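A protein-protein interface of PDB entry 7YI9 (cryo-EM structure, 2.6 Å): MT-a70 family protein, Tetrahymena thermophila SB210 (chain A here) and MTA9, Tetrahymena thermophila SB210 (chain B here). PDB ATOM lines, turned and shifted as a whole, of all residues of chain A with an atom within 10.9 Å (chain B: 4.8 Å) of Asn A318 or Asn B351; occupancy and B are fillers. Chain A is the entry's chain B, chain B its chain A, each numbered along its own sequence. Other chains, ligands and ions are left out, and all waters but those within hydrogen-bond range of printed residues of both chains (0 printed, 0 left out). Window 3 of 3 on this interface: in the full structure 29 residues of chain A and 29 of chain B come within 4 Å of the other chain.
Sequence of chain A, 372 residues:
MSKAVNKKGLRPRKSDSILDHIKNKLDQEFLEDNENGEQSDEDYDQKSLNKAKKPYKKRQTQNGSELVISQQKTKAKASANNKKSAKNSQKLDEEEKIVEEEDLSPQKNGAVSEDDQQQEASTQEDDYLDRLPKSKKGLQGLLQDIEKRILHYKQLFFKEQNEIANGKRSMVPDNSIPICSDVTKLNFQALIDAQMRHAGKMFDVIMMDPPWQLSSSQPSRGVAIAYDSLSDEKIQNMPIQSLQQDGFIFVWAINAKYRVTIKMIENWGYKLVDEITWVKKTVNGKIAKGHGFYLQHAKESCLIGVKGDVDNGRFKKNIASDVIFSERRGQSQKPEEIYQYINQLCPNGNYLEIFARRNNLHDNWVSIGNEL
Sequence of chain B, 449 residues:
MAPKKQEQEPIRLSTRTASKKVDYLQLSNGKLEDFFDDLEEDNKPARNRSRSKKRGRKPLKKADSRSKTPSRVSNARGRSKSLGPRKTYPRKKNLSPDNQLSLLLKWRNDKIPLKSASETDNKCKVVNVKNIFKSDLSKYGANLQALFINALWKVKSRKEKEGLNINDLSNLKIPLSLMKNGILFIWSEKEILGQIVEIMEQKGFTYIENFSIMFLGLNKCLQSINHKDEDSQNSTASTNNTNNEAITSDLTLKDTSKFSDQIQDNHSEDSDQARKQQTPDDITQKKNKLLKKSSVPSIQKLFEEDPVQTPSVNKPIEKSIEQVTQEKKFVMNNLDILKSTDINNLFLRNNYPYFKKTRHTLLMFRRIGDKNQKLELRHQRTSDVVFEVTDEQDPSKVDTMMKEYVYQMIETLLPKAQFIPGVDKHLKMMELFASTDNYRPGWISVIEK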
ATOM      1  N   PHE A 248     -10.775 -38.736 -17.899  1.00  0.00           N
ATOM      2  CA  PHE A 248     -11.569 -37.613 -17.432  1.00  0.00           C
ATOM      3  C   PHE A 248     -12.976 -37.674 -18.002  1.00  0.00           C
ATOM      4  O   PHE A 248     -13.227 -38.297 -19.034  1.00  0.00           O
ATOM      5  CB  PHE A 248     -10.928 -36.284 -17.845  1.00  0.00           C
ATOM      6  CG  PHE A 248      -9.840 -35.820 -16.932  1.00  0.00           C
ATOM      7  CD1 PHE A 248     -10.140 -35.109 -15.788  1.00  0.00           C
ATOM      8  CD2 PHE A 248      -8.517 -36.078 -17.224  1.00  0.00           C
ATOM      9  CE1 PHE A 248      -9.146 -34.676 -14.950  1.00  0.00           C
ATOM     10  CE2 PHE A 248      -7.518 -35.640 -16.390  1.00  0.00           C
ATOM     11  CZ  PHE A 248      -7.833 -34.945 -15.250  1.00  0.00           C
ATOM     12  N   VAL A 273     -13.044 -33.552  -8.878  1.00  0.00           N
ATOM     13  CA  VAL A 273     -11.769 -32.938  -8.520  1.00  0.00           C
ATOM     14  C   VAL A 273     -11.615 -31.518  -9.033  1.00  0.00           C
ATOM     15  O   VAL A 273     -10.713 -30.796  -8.570  1.00  0.00           O
ATOM     16  CB  VAL A 273     -10.594 -33.807  -9.017  1.00  0.00           C
ATOM     17  CG1 VAL A 273     -10.560 -35.127  -8.279  1.00  0.00           C
ATOM     18  CG2 VAL A 273     -10.700 -34.023 -10.512  1.00  0.00           C
ATOM     19  N   ASP A 274     -12.441 -31.052  -9.966  1.00  0.00           N
ATOM     20  CA  ASP A 274     -12.205 -29.764 -10.596  1.00  0.00           C
ATOM     21  C   ASP A 274     -13.509 -29.251 -11.178  1.00  0.00           C
ATOM     22  O   ASP A 274     -14.521 -29.954 -11.201  1.00  0.00           O
ATOM     23  CB  ASP A 274     -11.130 -29.866 -11.685  1.00  0.00           C
ATOM     24  CG  ASP A 274     -10.447 -28.542 -11.962  1.00  0.00           C
ATOM     25  OD1 ASP A 274     -11.136 -27.502 -11.987  1.00  0.00           O
ATOM     26  OD2 ASP A 274      -9.216 -28.542 -12.150  1.00  0.00           O
ATOM     27  N   ILE A 276     -14.549 -26.024 -14.221  1.00  0.00           N
ATOM     28  CA  ILE A 276     -14.157 -24.921 -15.090  1.00  0.00           C
ATOM     29  C   ILE A 276     -15.350 -23.995 -15.248  1.00  0.00           C
ATOM     30  O   ILE A 276     -16.442 -24.435 -15.622  1.00  0.00           O
ATOM     31  CB  ILE A 276     -13.660 -25.418 -16.460  1.00  0.00           C
ATOM     32  CG1 ILE A 276     -12.234 -25.949 -16.354  1.00  0.00           C
ATOM     33  CG2 ILE A 276     -13.702 -24.303 -17.487  1.00  0.00           C
ATOM     34  CD1 ILE A 276     -11.717 -26.536 -17.642  1.00  0.00           C
ATOM     35  N   VAL A 310      -4.900 -41.784 -14.126  1.00  0.00           N
ATOM     36  CA  VAL A 310      -5.055 -40.649 -15.027  1.00  0.00           C
ATOM     37  C   VAL A 310      -3.743 -39.918 -15.273  1.00  0.00           C
ATOM     38  O   VAL A 310      -3.679 -39.079 -16.183  1.00  0.00           O
ATOM     39  CB  VAL A 310      -6.125 -39.667 -14.504  1.00  0.00           C
ATOM     40  CG1 VAL A 310      -5.649 -38.965 -13.236  1.00  0.00           C
ATOM     41  CG2 VAL A 310      -6.571 -38.703 -15.577  1.00  0.00           C
ATOM     42  N   ASP A 311      -2.693 -40.209 -14.518  1.00  0.00           N
ATOM     43  CA  ASP A 311      -1.364 -39.663 -14.773  1.00  0.00           C
ATOM     44  C   ASP A 311      -0.496 -40.816 -15.272  1.00  0.00           C
ATOM     45  O   ASP A 311       0.206 -41.468 -14.498  1.00  0.00           O
ATOM     46  CB  ASP A 311      -0.788 -39.001 -13.523  1.00  0.00           C
ATOM     47  CG  ASP A 311      -1.018 -39.819 -12.268  1.00  0.00           C
ATOM     48  OD1 ASP A 311      -1.645 -40.893 -12.363  1.00  0.00           O
ATOM     49  OD2 ASP A 311      -0.577 -39.382 -11.185  1.00  0.00           O
ATOM     50  N   PHE A 315      -1.663 -37.326 -19.919  1.00  0.00           N
ATOM     51  CA  PHE A 315      -2.424 -36.199 -19.404  1.00  0.00           C
ATOM     52  C   PHE A 315      -1.465 -35.197 -18.776  1.00  0.00           C
ATOM     53  O   PHE A 315      -0.457 -35.575 -18.172  1.00  0.00           O
ATOM     54  CB  PHE A 315      -3.473 -36.648 -18.378  1.00  0.00           C
ATOM     55  CG  PHE A 315      -4.602 -37.446 -18.968  1.00  0.00           C
ATOM     56  CD1 PHE A 315      -5.728 -36.812 -19.462  1.00  0.00           C
ATOM     57  CD2 PHE A 315      -4.541 -38.828 -19.025  1.00  0.00           C
ATOM     58  CE1 PHE A 315      -6.770 -37.540 -20.000  1.00  0.00           C
ATOM     59  CE2 PHE A 315      -5.580 -39.559 -19.561  1.00  0.00           C
ATOM     60  CZ  PHE A 315      -6.694 -38.913 -20.051  1.00  0.00           C
ATOM     61  N   LYS A 316      -1.780 -33.913 -18.927  1.00  0.00           N
ATOM     62  CA  LYS A 316      -0.904 -32.836 -18.488  1.00  0.00           C
ATOM     63  C   LYS A 316      -1.527 -32.086 -17.319  1.00  0.00           C
ATOM     64  O   LYS A 316      -2.712 -31.741 -17.348  1.00  0.00           O
ATOM     65  CB  LYS A 316      -0.611 -31.866 -19.635  1.00  0.00           C
ATOM     66  CG  LYS A 316       0.039 -32.516 -20.846  1.00  0.00           C
ATOM     67  CD  LYS A 316       1.551 -32.519 -20.724  1.00  0.00           C
ATOM     68  CE  LYS A 316       2.180 -33.555 -21.638  1.00  0.00           C
ATOM     69  NZ  LYS A 316       2.248 -34.894 -20.991  1.00  0.00           N
ATOM     70  N   LYS A 317      -0.716 -31.825 -16.298  1.00  0.00           N
ATOM     71  CA  LYS A 317      -1.162 -31.201 -15.061  1.00  0.00           C
ATOM     72  C   LYS A 317      -0.791 -29.723 -15.029  1.00  0.00           C
ATOM     73  O   LYS A 317       0.261 -29.318 -15.529  1.00  0.00           O
ATOM     74  CB  LYS A 317      -0.545 -31.907 -13.853  1.00  0.00           C
ATOM     75  CG  LYS A 317      -1.083 -33.303 -13.604  1.00  0.00           C
ATOM     76  CD  LYS A 317      -0.553 -33.872 -12.300  1.00  0.00           C
ATOM     77  CE  LYS A 317       0.892 -34.321 -12.437  1.00  0.00           C
ATOM     78  NZ  LYS A 317       1.019 -35.539 -13.283  1.00  0.00           N
ATOM     79  N   ASN A 318      -1.673 -28.922 -14.425  1.00  0.00           N
ATOM     80  CA  ASN A 318      -1.420 -27.509 -14.142  1.00  0.00           C
ATOM     81  C   ASN A 318      -1.174 -26.731 -15.439  1.00  0.00           C
ATOM     82  O   ASN A 318      -0.117 -26.138 -15.660  1.00  0.00           O
ATOM     83  CB  ASN A 318      -0.240 -27.372 -13.171  1.00  0.00           C
ATOM     84  CG  ASN A 318      -0.097 -25.977 -12.611  1.00  0.00           C
ATOM     85  OD1 ASN A 318      -1.022 -25.175 -12.678  1.00  0.00           O
ATOM     86  ND2 ASN A 318       1.069 -25.679 -12.056  1.00  0.00           N
ATOM     87  N   ILE A 319      -2.192 -26.749 -16.294  1.00  0.00           N
ATOM     88  CA  ILE A 319      -2.061 -26.335 -17.685  1.00  0.00           C
ATOM     89  C   ILE A 319      -2.671 -24.958 -17.933  1.00  0.00           C
ATOM     90  O   ILE A 319      -1.974 -24.027 -18.336  1.00  0.00           O
ATOM     91  CB  ILE A 319      -2.665 -27.392 -18.638  1.00  0.00           C
ATOM     92  CG1 ILE A 319      -4.061 -27.808 -18.169  1.00  0.00           C
ATOM     93  CG2 ILE A 319      -1.743 -28.582 -18.752  1.00  0.00           C
ATOM     94  CD1 ILE A 319      -4.851 -28.555 -19.180  1.00  0.00           C
ATOM     95  N   ALA A 320      -3.972 -24.813 -17.710  1.00  0.00           N
ATOM     96  CA  ALA A 320      -4.676 -23.606 -18.111  1.00  0.00           C
ATOM     97  C   ALA A 320      -5.653 -23.215 -17.017  1.00  0.00           C
ATOM     98  O   ALA A 320      -5.987 -24.013 -16.141  1.00  0.00           O
ATOM     99  CB  ALA A 320      -5.410 -23.798 -19.441  1.00  0.00           C
ATOM    100  N   SER A 321      -6.113 -21.971 -17.079  1.00  0.00           N
ATOM    101  CA  SER A 321      -6.979 -21.462 -16.033  1.00  0.00           C
ATOM    102  C   SER A 321      -8.310 -22.206 -16.015  1.00  0.00           C
ATOM    103  O   SER A 321      -8.745 -22.793 -17.008  1.00  0.00           O
ATOM    104  CB  SER A 321      -7.220 -19.965 -16.212  1.00  0.00           C
ATOM    105  OG  SER A 321      -7.964 -19.700 -17.387  1.00  0.00           O
ATOM    106  N   ASP A 322      -8.948 -22.188 -14.849  1.00  0.00           N
ATOM    107  CA  ASP A 322     -10.290 -22.712 -14.667  1.00  0.00           C
ATOM    108  C   ASP A 322     -11.363 -21.694 -15.024  1.00  0.00           C
ATOM    109  O   ASP A 322     -12.531 -21.892 -14.680  1.00  0.00           O
ATOM    110  CB  ASP A 322     -10.468 -23.205 -13.227  1.00  0.00           C
ATOM    111  CG  ASP A 322     -10.326 -22.094 -12.196  1.00  0.00           C
ATOM    112  OD1 ASP A 322     -10.049 -20.938 -12.574  1.00  0.00           O
ATOM    113  OD2 ASP A 322     -10.494 -22.377 -10.993  1.00  0.00           O
ATOM    114  N   TYR A 341      -8.216 -26.327 -24.346  1.00  0.00           N
ATOM    115  CA  TYR A 341      -7.847 -26.749 -22.999  1.00  0.00           C
ATOM    116  C   TYR A 341      -7.741 -28.264 -22.908  1.00  0.00           C
ATOM    117  O   TYR A 341      -6.865 -28.789 -22.216  1.00  0.00           O
ATOM    118  CB  TYR A 341      -8.858 -26.223 -21.984  1.00  0.00           C
ATOM    119  CG  TYR A 341      -8.740 -24.748 -21.687  1.00  0.00           C
ATOM    120  CD1 TYR A 341      -7.732 -23.980 -22.253  1.00  0.00           C
ATOM    121  CD2 TYR A 341      -9.637 -24.122 -20.837  1.00  0.00           C
ATOM    122  CE1 TYR A 341      -7.627 -22.630 -21.983  1.00  0.00           C
ATOM    123  CE2 TYR A 341      -9.537 -22.777 -20.559  1.00  0.00           C
ATOM    124  CZ  TYR A 341      -8.534 -22.034 -21.135  1.00  0.00           C
ATOM    125  OH  TYR A 341      -8.439 -20.691 -20.854  1.00  0.00           O
ATOM    126  N   GLN A 344      -4.540 -29.239 -24.480  1.00  0.00           N
ATOM    127  CA  GLN A 344      -3.461 -29.022 -23.521  1.00  0.00           C
ATOM    128  C   GLN A 344      -3.449 -30.098 -22.441  1.00  0.00           C
ATOM    129  O   GLN A 344      -2.378 -30.495 -21.974  1.00  0.00           O
ATOM    130  CB  GLN A 344      -3.592 -27.638 -22.887  1.00  0.00           C
ATOM    131  CG  GLN A 344      -3.166 -26.498 -23.792  1.00  0.00           C
ATOM    132  CD  GLN A 344      -3.624 -25.149 -23.286  1.00  0.00           C
ATOM    133  OE1 GLN A 344      -3.046 -24.594 -22.354  1.00  0.00           O
ATOM    134  NE2 GLN A 344      -4.670 -24.610 -23.901  1.00  0.00           N
ATOM    135  N   LEU A 345      -4.628 -30.570 -22.034  1.00  0.00           N
ATOM    136  CA  LEU A 345      -4.728 -31.603 -21.009  1.00  0.00           C
ATOM    137  C   LEU A 345      -4.305 -32.960 -21.556  1.00  0.00           C
ATOM    138  O   LEU A 345      -3.452 -33.640 -20.977  1.00  0.00           O
ATOM    139  CB  LEU A 345      -6.159 -31.649 -20.471  1.00  0.00           C
ATOM    140  CG  LEU A 345      -6.554 -32.720 -19.454  1.00  0.00           C
ATOM    141  CD1 LEU A 345      -5.816 -32.533 -18.143  1.00  0.00           C
ATOM    142  CD2 LEU A 345      -8.054 -32.689 -19.234  1.00  0.00           C
ATOM    143  N   CYS A 346      -4.898 -33.375 -22.672  1.00  0.00           N
ATOM    144  CA  CYS A 346      -4.542 -34.628 -23.338  1.00  0.00           C
ATOM    145  C   CYS A 346      -4.124 -34.340 -24.772  1.00  0.00           C
ATOM    146  O   CYS A 346      -4.987 -34.146 -25.647  1.00  0.00           O
ATOM    147  CB  CYS A 346      -5.707 -35.615 -23.309  1.00  0.00           C
ATOM    148  SG  CYS A 346      -5.252 -37.305 -23.745  1.00  0.00           S
ATOM    149  N   SER B 157      -3.902 -27.399  -1.690  1.00  0.00           N
ATOM    150  CA  SER B 157      -3.715 -26.232  -2.545  1.00  0.00           C
ATOM    151  C   SER B 157      -3.075 -25.085  -1.772  1.00  0.00           C
ATOM    152  O   SER B 157      -2.119 -24.460  -2.243  1.00  0.00           O
ATOM    153  CB  SER B 157      -5.056 -25.803  -3.143  1.00  0.00           C
ATOM    154  OG  SER B 157      -4.931 -24.583  -3.849  1.00  0.00           O
ATOM    155  N   LYS B 159      -0.585 -24.102   0.602  1.00  0.00           N
ATOM    156  CA  LYS B 159       0.623 -24.792   1.024  1.00  0.00           C
ATOM    157  C   LYS B 159       1.250 -24.075   2.212  1.00  0.00           C
ATOM    158  O   LYS B 159       1.448 -22.856   2.173  1.00  0.00           O
ATOM    159  CB  LYS B 159       1.616 -24.882  -0.134  1.00  0.00           C
ATOM    160  CG  LYS B 159       1.079 -25.667  -1.317  1.00  0.00           C
ATOM    161  CD  LYS B 159       2.030 -25.639  -2.496  1.00  0.00           C
ATOM    162  CE  LYS B 159       1.442 -26.386  -3.682  1.00  0.00           C
ATOM    163  NZ  LYS B 159       0.214 -25.717  -4.197  1.00  0.00           N
ATOM    164  N   ARG B 349      -2.966 -16.991 -12.341  1.00  0.00           N
ATOM    165  CA  ARG B 349      -2.839 -18.413 -12.654  1.00  0.00           C
ATOM    166  C   ARG B 349      -2.061 -19.073 -11.521  1.00  0.00           C
ATOM    167  O   ARG B 349      -0.833 -19.175 -11.587  1.00  0.00           O
ATOM    168  CB  ARG B 349      -2.135 -18.625 -13.991  1.00  0.00           C
ATOM    169  CG  ARG B 349      -2.497 -17.642 -15.094  1.00  0.00           C
ATOM    170  CD  ARG B 349      -3.802 -17.994 -15.781  1.00  0.00           C
ATOM    171  NE  ARG B 349      -3.868 -17.405 -17.113  1.00  0.00           N
ATOM    172  CZ  ARG B 349      -4.986 -17.022 -17.715  1.00  0.00           C
ATOM    173  NH1 ARG B 349      -6.162 -17.128 -17.123  1.00  0.00           N
ATOM    174  NH2 ARG B 349      -4.920 -16.512 -18.942  1.00  0.00           N
ATOM    175  N   ASN B 350      -2.765 -19.525 -10.489  1.00  0.00           N
ATOM    176  CA  ASN B 350      -2.123 -20.205  -9.374  1.00  0.00           C
ATOM    177  C   ASN B 350      -2.059 -21.705  -9.630  1.00  0.00           C
ATOM    178  O   ASN B 350      -2.893 -22.271 -10.338  1.00  0.00           O
ATOM    179  CB  ASN B 350      -2.861 -19.932  -8.064  1.00  0.00           C
ATOM    180  CG  ASN B 350      -2.592 -18.546  -7.524  1.00  0.00           C
ATOM    181  OD1 ASN B 350      -3.439 -17.659  -7.608  1.00  0.00           O
ATOM    182  ND2 ASN B 350      -1.404 -18.351  -6.967  1.00  0.00           N
ATOM    183  N   ASN B 351      -1.057 -22.345  -9.031  1.00  0.00           N
ATOM    184  CA  ASN B 351      -0.810 -23.758  -9.278  1.00  0.00           C
ATOM    185  C   ASN B 351      -1.893 -24.624  -8.648  1.00  0.00           C
ATOM    186  O   ASN B 351      -2.241 -24.454  -7.476  1.00  0.00           O
ATOM    187  CB  ASN B 351       0.561 -24.154  -8.734  1.00  0.00           C
ATOM    188  CG  ASN B 351       1.688 -23.395  -9.394  1.00  0.00           C
ATOM    189  OD1 ASN B 351       1.456 -22.461 -10.158  1.00  0.00           O
ATOM    190  ND2 ASN B 351       2.917 -23.793  -9.103  1.00  0.00           N
ATOM    191  N   TYR B 352      -2.423 -25.556  -9.436  1.00  0.00           N
ATOM    192  CA  TYR B 352      -3.374 -26.562  -8.993  1.00  0.00           C
ATOM    193  C   TYR B 352      -3.096 -27.826  -9.790  1.00  0.00           C
ATOM    194  O   TYR B 352      -2.601 -27.739 -10.919  1.00  0.00           O
ATOM    195  CB  TYR B 352      -4.822 -26.093  -9.197  1.00  0.00           C
ATOM    196  CG  TYR B 352      -5.875 -27.015  -8.627  1.00  0.00           C
ATOM    197  CD1 TYR B 352      -6.130 -27.055  -7.262  1.00  0.00           C
ATOM    198  CD2 TYR B 352      -6.614 -27.848  -9.455  1.00  0.00           C
ATOM    199  CE1 TYR B 352      -7.091 -27.901  -6.740  1.00  0.00           C
ATOM    200  CE2 TYR B 352      -7.576 -28.694  -8.943  1.00  0.00           C
ATOM    201  CZ  TYR B 352      -7.812 -28.717  -7.587  1.00  0.00           C
ATOM    202  OH  TYR B 352      -8.769 -29.562  -7.079  1.00  0.00           O
ATOM    203  N   PRO B 353      -3.377 -29.008  -9.233  1.00  0.00           N
ATOM    204  CA  PRO B 353      -3.036 -30.249  -9.947  1.00  0.00           C
ATOM    205  C   PRO B 353      -3.670 -30.400 -11.320  1.00  0.00           C
ATOM    206  O   PRO B 353      -3.064 -31.039 -12.187  1.00  0.00           O
ATOM    207  CB  PRO B 353      -3.523 -31.338  -8.985  1.00  0.00           C
ATOM    208  CG  PRO B 353      -3.346 -30.734  -7.655  1.00  0.00           C
ATOM    209  CD  PRO B 353      -3.656 -29.269  -7.811  1.00  0.00           C
ATOM    210  N   TYR B 354      -4.862 -29.857 -11.561  1.00  0.00           N
ATOM    211  CA  TYR B 354      -5.559 -30.120 -12.814  1.00  0.00           C
ATOM    212  C   TYR B 354      -5.673 -28.885 -13.701  1.00  0.00           C
ATOM    213  O   TYR B 354      -5.180 -28.897 -14.831  1.00  0.00           O
ATOM    214  CB  TYR B 354      -6.943 -30.710 -12.516  1.00  0.00           C
ATOM    215  CG  TYR B 354      -6.877 -32.032 -11.784  1.00  0.00           C
ATOM    216  CD1 TYR B 354      -6.457 -33.183 -12.435  1.00  0.00           C
ATOM    217  CD2 TYR B 354      -7.212 -32.126 -10.442  1.00  0.00           C
ATOM    218  CE1 TYR B 354      -6.385 -34.390 -11.775  1.00  0.00           C
ATOM    219  CE2 TYR B 354      -7.142 -33.328  -9.773  1.00  0.00           C
ATOM    220  CZ  TYR B 354      -6.728 -34.457 -10.445  1.00  0.00           C
ATOM    221  OH  TYR B 354      -6.655 -35.662  -9.788  1.00  0.00           O
ATOM    222  N   LYS B 356      -5.314 -24.396 -13.614  1.00  0.00           N
ATOM    223  CA  LYS B 356      -4.795 -23.295 -12.812  1.00  0.00           C
ATOM    224  C   LYS B 356      -5.924 -22.546 -12.115  1.00  0.00           C
ATOM    225  O   LYS B 356      -6.997 -22.331 -12.684  1.00  0.00           O
ATOM    226  CB  LYS B 356      -3.988 -22.343 -13.691  1.00  0.00           C
ATOM    227  CG  LYS B 356      -2.553 -22.783 -13.867  1.00  0.00           C
ATOM    228  CD  LYS B 356      -1.863 -22.045 -14.986  1.00  0.00           C
ATOM    229  CE  LYS B 356      -0.385 -22.369 -14.999  1.00  0.00           C
ATOM    230  NZ  LYS B 356       0.272 -21.947 -13.734  1.00  0.00           N
ATOM    231  N   LYS B 357      -5.673 -22.152 -10.868  1.00  0.00           N
ATOM    232  CA  LYS B 357      -6.686 -21.504 -10.046  1.00  0.00           C
ATOM    233  C   LYS B 357      -6.790 -20.023 -10.381  1.00  0.00           C
ATOM    234  O   LYS B 357      -5.786 -19.308 -10.405  1.00  0.00           O
ATOM    235  CB  LYS B 357      -6.363 -21.678  -8.564  1.00  0.00           C
ATOM    236  CG  LYS B 357      -6.485 -23.097  -8.063  1.00  0.00           C
ATOM    237  CD  LYS B 357      -6.054 -23.205  -6.617  1.00  0.00           C
ATOM    238  CE  LYS B 357      -7.077 -22.572  -5.697  1.00  0.00           C
ATOM    239  NZ  LYS B 357      -6.761 -22.821  -4.267  1.00  0.00           N
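Asn A318 touches just these residues of chain B: Asn B351 (3.6 Å), Tyr B352 (3.3 Å), Pro B353 (3.4 Å), Tyr B354 (3.5 Å) and Lys B356 (3.1 Å). Asn B351 touches one residue of chain A. No residue of chain A comes within 4 Å of Asn B350. Printed residues of chain A within 4 Å of Tyr B354: Phe A248 (3.6 Å), Val A273 (3.6 Å), Asp A274 (3.2 Å), Asn A318 (3.5 Å) and Ile A319 (3.7 Å). Of the printed residues of chain B, Asp A274 touches Tyr B352 (3.6 Å) and Tyr B354 (3.2 Å). Of the printed residues of chain B, Ser A321 touches Arg B349 (3.2 Å) and Lys B356 (3.5 Å). The nearest residue of chain B that does not touch Asn A318 is Asn B350 (4.2 Å). The nearest residue of chain A that does not touch Asn B351 is Ile A319 (7.8 Å). The nearest printed residue of chain B that does not touch Lys A317 is Tyr B354 (4.5 Å).
Among the printed residues, pairs that only touch across the chains: Phe A248 with Tyr B354, Val A273 with Tyr B354, Asp A274 with Tyr B352, Asp A274 with Tyr B354, Lys A317 with Pro B353, Asn A318 with Asn B351, Asn A318 with Tyr B354, Asn A318 with Lys B356, Ile A319 with Tyr B354, Ile A319 with Lys B356 and Ser A321 with Lys B356.
The backbone carbonyl oxygen (O) of Ala A320 lies within hydrogen-bond range of the backbone NH (N) of Lys B356 (2.6 Å). The guanidinium group (NH1) of Arg B349 is in hydrogen-bond range of the side-chain hydroxyl (OG) of Ser A321 (3.2 Å). The backbone carbonyl oxygen (O) of Lys B356 sits at hydrogen-bond distance from the backbone NH (N) of Asp A322. The backbone carbonyl oxygen (O) of Pro B353 lies within hydrogen-bond range of the backbone NH (N) of Asn A318, 3.4 Å away. The side-chain hydroxyl (OH) of Tyr B352 sits at hydrogen-bond distance from the backbone carbonyl oxygen (O) of Val A273 (2.7 Å). O of Tyr B352 lies close to OD1 of Asn A318 (3.5 Å).
Of the 18 printed residues of chain A, 9 touch a printed residue of chain B. Printed residues of chain A that touch a printed residue of chain B: Phe A248, Val A273, Asp A274, Lys A317, Asn A318, Ile A319, Ala A320, Ser A321 and Asp A322. Hydrophobic or aromatic side chains of chain A that line the printed part of chain B: Phe A248, Val A273 and Ile A319. Hydrophobic or aromatic side chains of chain B that line the printed part of chain A: Tyr B352 and Tyr B354. Among the printed residues, 17 pairs touch across the chains. Among the printed residues, no Asp or Glu carboxylate lies within 4 Å of a Lys or Arg side-chain nitrogen of the other chain.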
